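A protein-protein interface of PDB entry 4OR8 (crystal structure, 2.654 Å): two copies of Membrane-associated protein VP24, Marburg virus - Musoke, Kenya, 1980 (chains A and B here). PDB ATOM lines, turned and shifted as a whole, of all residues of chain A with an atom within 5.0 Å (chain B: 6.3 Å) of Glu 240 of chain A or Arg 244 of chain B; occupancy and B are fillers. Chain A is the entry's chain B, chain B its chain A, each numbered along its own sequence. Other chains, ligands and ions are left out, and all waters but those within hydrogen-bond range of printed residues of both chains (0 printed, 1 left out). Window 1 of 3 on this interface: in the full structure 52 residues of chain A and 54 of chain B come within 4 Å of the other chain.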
ATOM      1  N   PHE A 179     -11.658  11.307   6.750  1.00  0.00           N
ATOM      2  CA  PHE A 179     -12.159  12.188   7.796  1.00  0.00           C
ATOM      3  C   PHE A 179     -12.188  13.651   7.360  1.00  0.00           C
ATOM      4  O   PHE A 179     -12.634  14.521   8.108  1.00  0.00           O
ATOM      5  CB  PHE A 179     -11.350  12.021   9.080  1.00  0.00           C
ATOM      6  CG  PHE A 179     -11.702  10.784   9.846  1.00  0.00           C
ATOM      7  CD1 PHE A 179     -12.801  10.771  10.687  1.00  0.00           C
ATOM      8  CD2 PHE A 179     -10.948   9.631   9.717  1.00  0.00           C
ATOM      9  CE1 PHE A 179     -13.137   9.633  11.391  1.00  0.00           C
ATOM     10  CE2 PHE A 179     -11.281   8.488  10.419  1.00  0.00           C
ATOM     11  CZ  PHE A 179     -12.378   8.490  11.258  1.00  0.00           C
ATOM     12  N   VAL A 183     -20.113  15.091   6.859  1.00  0.00           N
ATOM     13  CA  VAL A 183     -21.356  14.344   6.946  1.00  0.00           C
ATOM     14  C   VAL A 183     -22.324  14.978   5.953  1.00  0.00           C
ATOM     15  O   VAL A 183     -22.176  16.150   5.613  1.00  0.00           O
ATOM     16  CB  VAL A 183     -21.930  14.401   8.376  1.00  0.00           C
ATOM     17  CG1 VAL A 183     -23.154  13.517   8.505  1.00  0.00           C
ATOM     18  CG2 VAL A 183     -20.878  13.965   9.370  1.00  0.00           C
ATOM     19  N   ARG A 206     -19.982   9.604   4.345  1.00  0.00           N
ATOM     20  CA  ARG A 206     -19.915   9.840   5.780  1.00  0.00           C
ATOM     21  C   ARG A 206     -21.273  10.242   6.350  1.00  0.00           C
ATOM     22  O   ARG A 206     -21.886  11.216   5.908  1.00  0.00           O
ATOM     23  CB  ARG A 206     -18.869  10.900   6.122  1.00  0.00           C
ATOM     24  CG  ARG A 206     -18.722  11.121   7.612  1.00  0.00           C
ATOM     25  CD  ARG A 206     -17.589  12.074   7.936  1.00  0.00           C
ATOM     26  NE  ARG A 206     -17.289  12.056   9.366  1.00  0.00           N
ATOM     27  CZ  ARG A 206     -16.249  12.665   9.922  1.00  0.00           C
ATOM     28  NH1 ARG A 206     -15.396  13.351   9.171  1.00  0.00           N
ATOM     29  NH2 ARG A 206     -16.059  12.586  11.231  1.00  0.00           N
ATOM     30  N   ASN A 208     -23.541  10.425  10.353  1.00  0.00           N
ATOM     31  CA  ASN A 208     -23.278  10.702  11.760  1.00  0.00           C
ATOM     32  C   ASN A 208     -22.705   9.502  12.508  1.00  0.00           C
ATOM     33  O   ASN A 208     -21.928   9.660  13.452  1.00  0.00           O
ATOM     34  CB  ASN A 208     -24.547  11.190  12.461  1.00  0.00           C
ATOM     35  CG  ASN A 208     -24.958  12.578  12.022  1.00  0.00           C
ATOM     36  OD1 ASN A 208     -24.113  13.421  11.723  1.00  0.00           O
ATOM     37  ND2 ASN A 208     -26.264  12.824  11.981  1.00  0.00           N
ATOM     38  N   MET A 209     -23.091   8.305  12.080  1.00  0.00           N
ATOM     39  CA  MET A 209     -22.698   7.081  12.775  1.00  0.00           C
ATOM     40  C   MET A 209     -21.350   6.555  12.306  1.00  0.00           C
ATOM     41  O   MET A 209     -20.713   5.750  12.985  1.00  0.00           O
ATOM     42  CB  MET A 209     -23.769   6.004  12.603  1.00  0.00           C
ATOM     43  CG  MET A 209     -25.084   6.351  13.271  1.00  0.00           C
ATOM     44  SD  MET A 209     -26.259   4.989  13.242  1.00  0.00           S
ATOM     45  CE  MET A 209     -25.285   3.685  13.989  1.00  0.00           C
ATOM     46  N   GLY A 210     -20.915   7.017  11.144  1.00  0.00           N
ATOM     47  CA  GLY A 210     -19.663   6.563  10.576  1.00  0.00           C
ATOM     48  C   GLY A 210     -19.690   6.644   9.067  1.00  0.00           C
ATOM     49  O   GLY A 210     -20.159   7.625   8.499  1.00  0.00           O
ATOM     50  N   PHE A 211     -19.195   5.603   8.413  1.00  0.00           N
ATOM     51  CA  PHE A 211     -19.095   5.612   6.964  1.00  0.00           C
ATOM     52  C   PHE A 211     -19.966   4.540   6.334  1.00  0.00           C
ATOM     53  O   PHE A 211     -19.791   3.352   6.587  1.00  0.00           O
ATOM     54  CB  PHE A 211     -17.639   5.449   6.532  1.00  0.00           C
ATOM     55  CG  PHE A 211     -16.741   6.544   7.026  1.00  0.00           C
ATOM     56  CD1 PHE A 211     -16.622   7.727   6.319  1.00  0.00           C
ATOM     57  CD2 PHE A 211     -16.030   6.396   8.204  1.00  0.00           C
ATOM     58  CE1 PHE A 211     -15.801   8.742   6.771  1.00  0.00           C
ATOM     59  CE2 PHE A 211     -15.206   7.406   8.663  1.00  0.00           C
ATOM     60  CZ  PHE A 211     -15.092   8.582   7.945  1.00  0.00           C
ATOM     61  N   VAL A 238     -19.560   1.154   8.461  1.00  0.00           N
ATOM     62  CA  VAL A 238     -18.359   1.080   9.278  1.00  0.00           C
ATOM     63  C   VAL A 238     -18.350   2.217  10.293  1.00  0.00           C
ATOM     64  O   VAL A 238     -18.369   3.390   9.924  1.00  0.00           O
ATOM     65  CB  VAL A 238     -17.072   1.123   8.432  1.00  0.00           C
ATOM     66  CG1 VAL A 238     -15.853   1.119   9.336  1.00  0.00           C
ATOM     67  CG2 VAL A 238     -17.021  -0.059   7.476  1.00  0.00           C
ATOM     68  N   ALA A 239     -18.334   1.856  11.574  1.00  0.00           N
ATOM     69  CA  ALA A 239     -18.352   2.834  12.653  1.00  0.00           C
ATOM     70  C   ALA A 239     -17.097   3.690  12.634  1.00  0.00           C
ATOM     71  O   ALA A 239     -16.006   3.208  12.337  1.00  0.00           O
ATOM     72  CB  ALA A 239     -18.498   2.142  13.988  1.00  0.00           C
ATOM     73  N   GLU A 240     -17.269   4.962  12.963  1.00  0.00           N
ATOM     74  CA  GLU A 240     -16.197   5.947  12.918  1.00  0.00           C
ATOM     75  C   GLU A 240     -14.960   5.529  13.712  1.00  0.00           C
ATOM     76  O   GLU A 240     -13.832   5.726  13.260  1.00  0.00           O
ATOM     77  CB  GLU A 240     -16.728   7.283  13.435  1.00  0.00           C
ATOM     78  CG  GLU A 240     -15.814   8.465  13.215  1.00  0.00           C
ATOM     79  CD  GLU A 240     -16.483   9.774  13.588  1.00  0.00           C
ATOM     80  OE1 GLU A 240     -17.722   9.779  13.753  1.00  0.00           O
ATOM     81  OE2 GLU A 240     -15.775  10.795  13.723  1.00  0.00           O
ATOM     82  N   ALA A 241     -15.179   4.946  14.889  1.00  0.00           N
ATOM     83  CA  ALA A 241     -14.090   4.543  15.776  1.00  0.00           C
ATOM     84  C   ALA A 241     -13.145   3.520  15.137  1.00  0.00           C
ATOM     85  O   ALA A 241     -11.945   3.508  15.419  1.00  0.00           O
ATOM     86  CB  ALA A 241     -14.645   4.012  17.080  1.00  0.00           C
ATOM     87  N   VAL A 242     -13.693   2.666  14.280  1.00  0.00           N
ATOM     88  CA  VAL A 242     -12.908   1.661  13.570  1.00  0.00           C
ATOM     89  C   VAL A 242     -11.741   2.282  12.810  1.00  0.00           C
ATOM     90  O   VAL A 242     -10.621   1.768  12.835  1.00  0.00           O
ATOM     91  CB  VAL A 242     -13.786   0.886  12.566  1.00  0.00           C
ATOM     92  CG1 VAL A 242     -12.931  -0.018  11.691  1.00  0.00           C
ATOM     93  CG2 VAL A 242     -14.855   0.087  13.298  1.00  0.00           C
ATOM     94  N   LEU A 243     -12.010   3.400  12.143  1.00  0.00           N
ATOM     95  CA  LEU A 243     -11.008   4.057  11.313  1.00  0.00           C
ATOM     96  C   LEU A 243     -10.258   5.161  12.055  1.00  0.00           C
ATOM     97  O   LEU A 243      -9.106   5.453  11.740  1.00  0.00           O
ATOM     98  CB  LEU A 243     -11.657   4.620  10.048  1.00  0.00           C
ATOM     99  CG  LEU A 243     -12.485   3.613   9.250  1.00  0.00           C
ATOM    100  CD1 LEU A 243     -13.136   4.273   8.055  1.00  0.00           C
ATOM    101  CD2 LEU A 243     -11.620   2.444   8.807  1.00  0.00           C
ATOM    102  N   ARG A 244     -10.909   5.770  13.041  1.00  0.00           N
ATOM    103  CA  ARG A 244     -10.293   6.866  13.786  1.00  0.00           C
ATOM    104  C   ARG A 244      -9.097   6.378  14.597  1.00  0.00           C
ATOM    105  O   ARG A 244      -8.142   7.117  14.829  1.00  0.00           O
ATOM    106  CB  ARG A 244     -11.315   7.545  14.696  1.00  0.00           C
ATOM    107  CG  ARG A 244     -10.777   8.766  15.408  1.00  0.00           C
ATOM    108  CD  ARG A 244     -11.868   9.486  16.165  1.00  0.00           C
ATOM    109  NE  ARG A 244     -12.877  10.056  15.278  1.00  0.00           N
ATOM    110  CZ  ARG A 244     -12.696  11.158  14.555  1.00  0.00           C
ATOM    111  NH1 ARG A 244     -11.538  11.801  14.598  1.00  0.00           N
ATOM    112  NH2 ARG A 244     -13.670  11.613  13.783  1.00  0.00           N
ATOM    113  N   PHE B 179     -15.757  18.944  19.747  1.00  0.00           N
ATOM    114  CA  PHE B 179     -15.216  18.250  18.589  1.00  0.00           C
ATOM    115  C   PHE B 179     -13.876  18.827  18.150  1.00  0.00           C
ATOM    116  O   PHE B 179     -13.238  18.299  17.240  1.00  0.00           O
ATOM    117  CB  PHE B 179     -16.219  18.246  17.435  1.00  0.00           C
ATOM    118  CG  PHE B 179     -17.236  17.145  17.528  1.00  0.00           C
ATOM    119  CD1 PHE B 179     -16.970  15.895  16.998  1.00  0.00           C
ATOM    120  CD2 PHE B 179     -18.450  17.355  18.158  1.00  0.00           C
ATOM    121  CE1 PHE B 179     -17.897  14.879  17.089  1.00  0.00           C
ATOM    122  CE2 PHE B 179     -19.386  16.338  18.248  1.00  0.00           C
ATOM    123  CZ  PHE B 179     -19.108  15.101  17.714  1.00  0.00           C
ATOM    124  N   ARG B 206     -12.112  12.896  25.177  1.00  0.00           N
ATOM    125  CA  ARG B 206     -12.423  12.392  23.843  1.00  0.00           C
ATOM    126  C   ARG B 206     -11.609  11.155  23.489  1.00  0.00           C
ATOM    127  O   ARG B 206     -10.390  11.219  23.334  1.00  0.00           O
ATOM    128  CB  ARG B 206     -12.218  13.470  22.775  1.00  0.00           C
ATOM    129  CG  ARG B 206     -12.549  12.977  21.369  1.00  0.00           C
ATOM    130  CD  ARG B 206     -12.539  14.089  20.336  1.00  0.00           C
ATOM    131  NE  ARG B 206     -13.042  13.621  19.043  1.00  0.00           N
ATOM    132  CZ  ARG B 206     -13.120  14.375  17.950  1.00  0.00           C
ATOM    133  NH1 ARG B 206     -12.727  15.642  17.983  1.00  0.00           N
ATOM    134  NH2 ARG B 206     -13.589  13.863  16.822  1.00  0.00           N
ATOM    135  N   ASN B 208     -11.638   7.385  20.927  1.00  0.00           N
ATOM    136  CA  ASN B 208     -12.015   6.995  19.571  1.00  0.00           C
ATOM    137  C   ASN B 208     -13.510   6.748  19.415  1.00  0.00           C
ATOM    138  O   ASN B 208     -14.088   7.033  18.367  1.00  0.00           O
ATOM    139  CB  ASN B 208     -11.240   5.751  19.132  1.00  0.00           C
ATOM    140  CG  ASN B 208      -9.781   6.041  18.857  1.00  0.00           C
ATOM    141  OD1 ASN B 208      -9.431   7.113  18.365  1.00  0.00           O
ATOM    142  ND2 ASN B 208      -8.918   5.082  19.171  1.00  0.00           N
ATOM    143  N   ALA B 239     -21.647   8.287  22.881  1.00  0.00           N
ATOM    144  CA  ALA B 239     -21.221   7.953  21.526  1.00  0.00           C
ATOM    145  C   ALA B 239     -21.137   9.198  20.655  1.00  0.00           C
ATOM    146  O   ALA B 239     -21.981  10.089  20.742  1.00  0.00           O
ATOM    147  CB  ALA B 239     -22.160   6.942  20.912  1.00  0.00           C
ATOM    148  N   GLU B 240     -20.111   9.244  19.812  1.00  0.00           N
ATOM    149  CA  GLU B 240     -19.832  10.407  18.980  1.00  0.00           C
ATOM    150  C   GLU B 240     -21.012  10.808  18.093  1.00  0.00           C
ATOM    151  O   GLU B 240     -21.183  11.983  17.774  1.00  0.00           O
ATOM    152  CB  GLU B 240     -18.591  10.147  18.125  1.00  0.00           C
ATOM    153  CG  GLU B 240     -17.941  11.402  17.581  1.00  0.00           C
ATOM    154  CD  GLU B 240     -16.657  11.110  16.829  1.00  0.00           C
ATOM    155  OE1 GLU B 240     -16.284   9.921  16.718  1.00  0.00           O
ATOM    156  OE2 GLU B 240     -16.022  12.074  16.351  1.00  0.00           O
ATOM    157  N   ALA B 241     -21.829   9.831  17.708  1.00  0.00           N
ATOM    158  CA  ALA B 241     -22.962  10.075  16.821  1.00  0.00           C
ATOM    159  C   ALA B 241     -24.043  10.924  17.483  1.00  0.00           C
ATOM    160  O   ALA B 241     -24.738  11.690  16.812  1.00  0.00           O
ATOM    161  CB  ALA B 241     -23.546   8.757  16.339  1.00  0.00           C
ATOM    162  N   VAL B 242     -24.179  10.778  18.796  1.00  0.00           N
ATOM    163  CA  VAL B 242     -25.165  11.521  19.571  1.00  0.00           C
ATOM    164  C   VAL B 242     -24.955  13.021  19.432  1.00  0.00           C
ATOM    165  O   VAL B 242     -25.910  13.786  19.293  1.00  0.00           O
ATOM    166  CB  VAL B 242     -25.071  11.167  21.070  1.00  0.00           C
ATOM    167  CG1 VAL B 242     -26.078  11.977  21.873  1.00  0.00           C
ATOM    168  CG2 VAL B 242     -25.278   9.676  21.281  1.00  0.00           C
ATOM    169  N   LEU B 243     -23.696  13.439  19.465  1.00  0.00           N
ATOM    170  CA  LEU B 243     -23.372  14.857  19.441  1.00  0.00           C
ATOM    171  C   LEU B 243     -23.084  15.348  18.026  1.00  0.00           C
ATOM    172  O   LEU B 243     -23.355  16.505  17.702  1.00  0.00           O
ATOM    173  CB  LEU B 243     -22.182  15.142  20.358  1.00  0.00           C
ATOM    174  CG  LEU B 243     -22.306  14.566  21.771  1.00  0.00           C
ATOM    175  CD1 LEU B 243     -21.032  14.803  22.561  1.00  0.00           C
ATOM    176  CD2 LEU B 243     -23.503  15.154  22.497  1.00  0.00           C
ATOM    177  N   ARG B 244     -22.537  14.468  17.191  1.00  0.00           N
ATOM    178  CA  ARG B 244     -22.195  14.816  15.812  1.00  0.00           C
ATOM    179  C   ARG B 244     -23.423  15.335  15.077  1.00  0.00           C
ATOM    180  O   ARG B 244     -23.365  16.342  14.373  1.00  0.00           O
ATOM    181  CB  ARG B 244     -21.616  13.601  15.083  1.00  0.00           C
ATOM    182  CG  ARG B 244     -21.346  13.819  13.600  1.00  0.00           C
ATOM    183  CD  ARG B 244     -20.040  14.555  13.365  1.00  0.00           C
ATOM    184  NE  ARG B 244     -18.898  13.786  13.848  1.00  0.00           N
ATOM    185  CZ  ARG B 244     -17.632  14.176  13.742  1.00  0.00           C
ATOM    186  NH1 ARG B 244     -17.334  15.330  13.160  1.00  0.00           N
ATOM    187  NH2 ARG B 244     -16.662  13.408  14.216  1.00  0.00           N
ATOM    188  N   GLU B 245     -24.539  14.643  15.274  1.00  0.00           N
ATOM    189  CA  GLU B 245     -25.818  15.016  14.686  1.00  0.00           C
ATOM    190  C   GLU B 245     -26.233  16.430  15.082  1.00  0.00           C
ATOM    191  O   GLU B 245     -26.891  17.129  14.314  1.00  0.00           O
ATOM    192  CB  GLU B 245     -26.885  14.014  15.129  1.00  0.00           C
ATOM    193  CG  GLU B 245     -28.277  14.284  14.594  1.00  0.00           C
ATOM    194  CD  GLU B 245     -29.251  13.184  14.968  1.00  0.00           C
ATOM    195  OE1 GLU B 245     -28.802  12.156  15.520  1.00  0.00           O
ATOM    196  OE2 GLU B 245     -30.463  13.349  14.714  1.00  0.00           O
ATOM    197  N   HIS B 246     -25.837  16.849  16.279  1.00  0.00           N
ATOM    198  CA  HIS B 246     -26.218  18.154  16.803  1.00  0.00           C
ATOM    199  C   HIS B 246     -25.006  19.048  17.038  1.00  0.00           C
ATOM    200  O   HIS B 246     -24.996  19.853  17.967  1.00  0.00           O
ATOM    201  CB  HIS B 246     -26.977  17.990  18.121  1.00  0.00           C
ATOM    202  CG  HIS B 246     -28.146  17.060  18.033  1.00  0.00           C
ATOM    203  ND1 HIS B 246     -29.325  17.403  17.409  1.00  0.00           N
ATOM    204  CD2 HIS B 246     -28.319  15.800  18.499  1.00  0.00           C
ATOM    205  CE1 HIS B 246     -30.174  16.393  17.490  1.00  0.00           C
ATOM    206  NE2 HIS B 246     -29.588  15.409  18.147  1.00  0.00           N
ATOM    207  N   SER B 247     -23.984  18.906  16.201  1.00  0.00           N
ATOM    208  CA  SER B 247     -22.753  19.668  16.383  1.00  0.00           C
ATOM    209  C   SER B 247     -22.672  20.847  15.423  1.00  0.00           C
ATOM    210  O   SER B 247     -21.977  21.829  15.688  1.00  0.00           O
ATOM    211  CB  SER B 247     -21.534  18.762  16.210  1.00  0.00           C
ATOM    212  OG  SER B 247     -21.578  18.088  14.965  1.00  0.00           O
ATOM    213  N   GLN B 248     -23.386  20.744  14.309  1.00  0.00           N
ATOM    214  CA  GLN B 248     -23.414  21.812  13.318  1.00  0.00           C
ATOM    215  C   GLN B 248     -24.688  22.643  13.444  1.00  0.00           C
ATOM    216  O   GLN B 248     -25.701  22.166  13.957  1.00  0.00           O
ATOM    217  CB  GLN B 248     -23.289  21.229  11.910  1.00  0.00           C
ATOM    218  CG  GLN B 248     -21.954  20.553  11.645  1.00  0.00           C
ATOM    219  CD  GLN B 248     -20.800  21.537  11.618  1.00  0.00           C
ATOM    220  OE1 GLN B 248     -19.688  21.220  12.044  1.00  0.00           O
ATOM    221  NE2 GLN B 248     -21.058  22.737  11.112  1.00  0.00           N
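OE2 of Glu 240 of chain B lies within salt-bridge range of NH2 of Arg 244 of chain A (3.5 Å).
The guanidinium group of Arg 244 of chain B lies within salt-bridge range of the side-chain carboxylate of Glu 240 of chain A.
The guanidinium group of Arg 206 of chain A sits close to the guanidinium group of Arg 244 of chain B (3.2 Å).
The side-chain carboxylate (OE2) of Glu 240 of chain A sits close to the side-chain carboxylate (OE2) of Glu 240 of chain B (2.9 Å).
Among the printed residues, merely in contact across the chains: Asn 208 of chain A with Ala 241 of chain B (3.4 Å), Asn 208 of chain A with Arg 244 of chain B (3.4 Å), Asn 208 of chain A with Glu 245 of chain B (3.4 Å), Ala 241 of chain A with Asn 208 of chain B (3.3 Å), Arg 244 of chain A with Arg 206 of chain B (3.6 Å), Arg 244 of chain A with Asn 208 of chain B (3.6 Å) and Arg 244 of chain A with Arg 244 of chain B (3.5 Å).
The backbone carbonyl oxygen of Phe 179 of chain B sits at hydrogen-bond distance from the guanidinium group of Arg 206 of chain B (2.8 Å).
NH2 of Arg 206 of chain B lies within salt-bridge range of OE2 of Glu 240 of chain B.
O of Arg 244 of chain B lies within hydrogen-bond range of OG of Ser 247 of chain B (2.6 Å).
The guanidinium group (NH1) of Arg 206 of chain A lies within hydrogen-bond range of the backbone carbonyl oxygen (O) of Phe 179 of chain A (3.2 Å).
OE2 of Glu 240 of chain A is in salt-bridge range of NH2 of Arg 206 of chain A (3.1 Å).
OE2 of Glu 240 of chain A is in salt-bridge range of NE of Arg 244 of chain A, at 3.4 Å.
Arg 206 of chain A touches Arg 244 of chain B, and with the chains exchanged Arg 244 of chain A touches Arg 206 of chain B.
Asn 208 of chain A touches Arg 244 of chain B, and with the chains exchanged Arg 244 of chain A touches Asn 208 of chain B.
Glu 240 of chain A touches Arg 244 of chain B, and with the chains exchanged Arg 244 of chain A touches Glu 240 of chain B.
Arg 244 of chain A touches its own counterpart, Arg 244 of chain B.
Of the 11 pairs that touch across the chains among the printed residues, 10 have their exchanged pair printed and touching as well.
Of the 13 printed residues of chain B, 6 touch a printed residue of chain A.
Hydrophobic or aromatic side chains of chain B that line the printed part of chain A: Ala 241.
Printed residues of chain A that touch a printed residue of chain B: Arg 206, Asn 208, Glu 240, Ala 241 and Arg 244.
Hydrophobic or aromatic side chains of chain A that line the printed part of chain B: Ala 241.
Of the printed residues of chain B, Asn 208 of chain A touches Ala 241 (3.4 Å), Arg 244 (3.4 Å) and Glu 245 (3.4 Å).
Glu 240 of chain A touches just these residues of chain B: Glu 240 (2.9 Å) and Arg 244 (2.8 Å).
Of the printed residues of chain B, Ala 241 of chain A touches Asn 208 (3.3 Å).
Of the printed residues of chain B, Arg 244 of chain A touches Arg 206 (3.6 Å), Asn 208 (3.6 Å), Glu 240 (3.5 Å) and Arg 244 (3.5 Å).
Of the printed residues of chain A, Glu 240 of chain B touches Glu 240 and Arg 244.
Of the printed residues of chain A, Ala 241 of chain B touches Asn 208 (3.4 Å).
The nearest residue of chain A that does not touch Arg 244 of chain B is Val 183 of chain A (4.1 Å).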
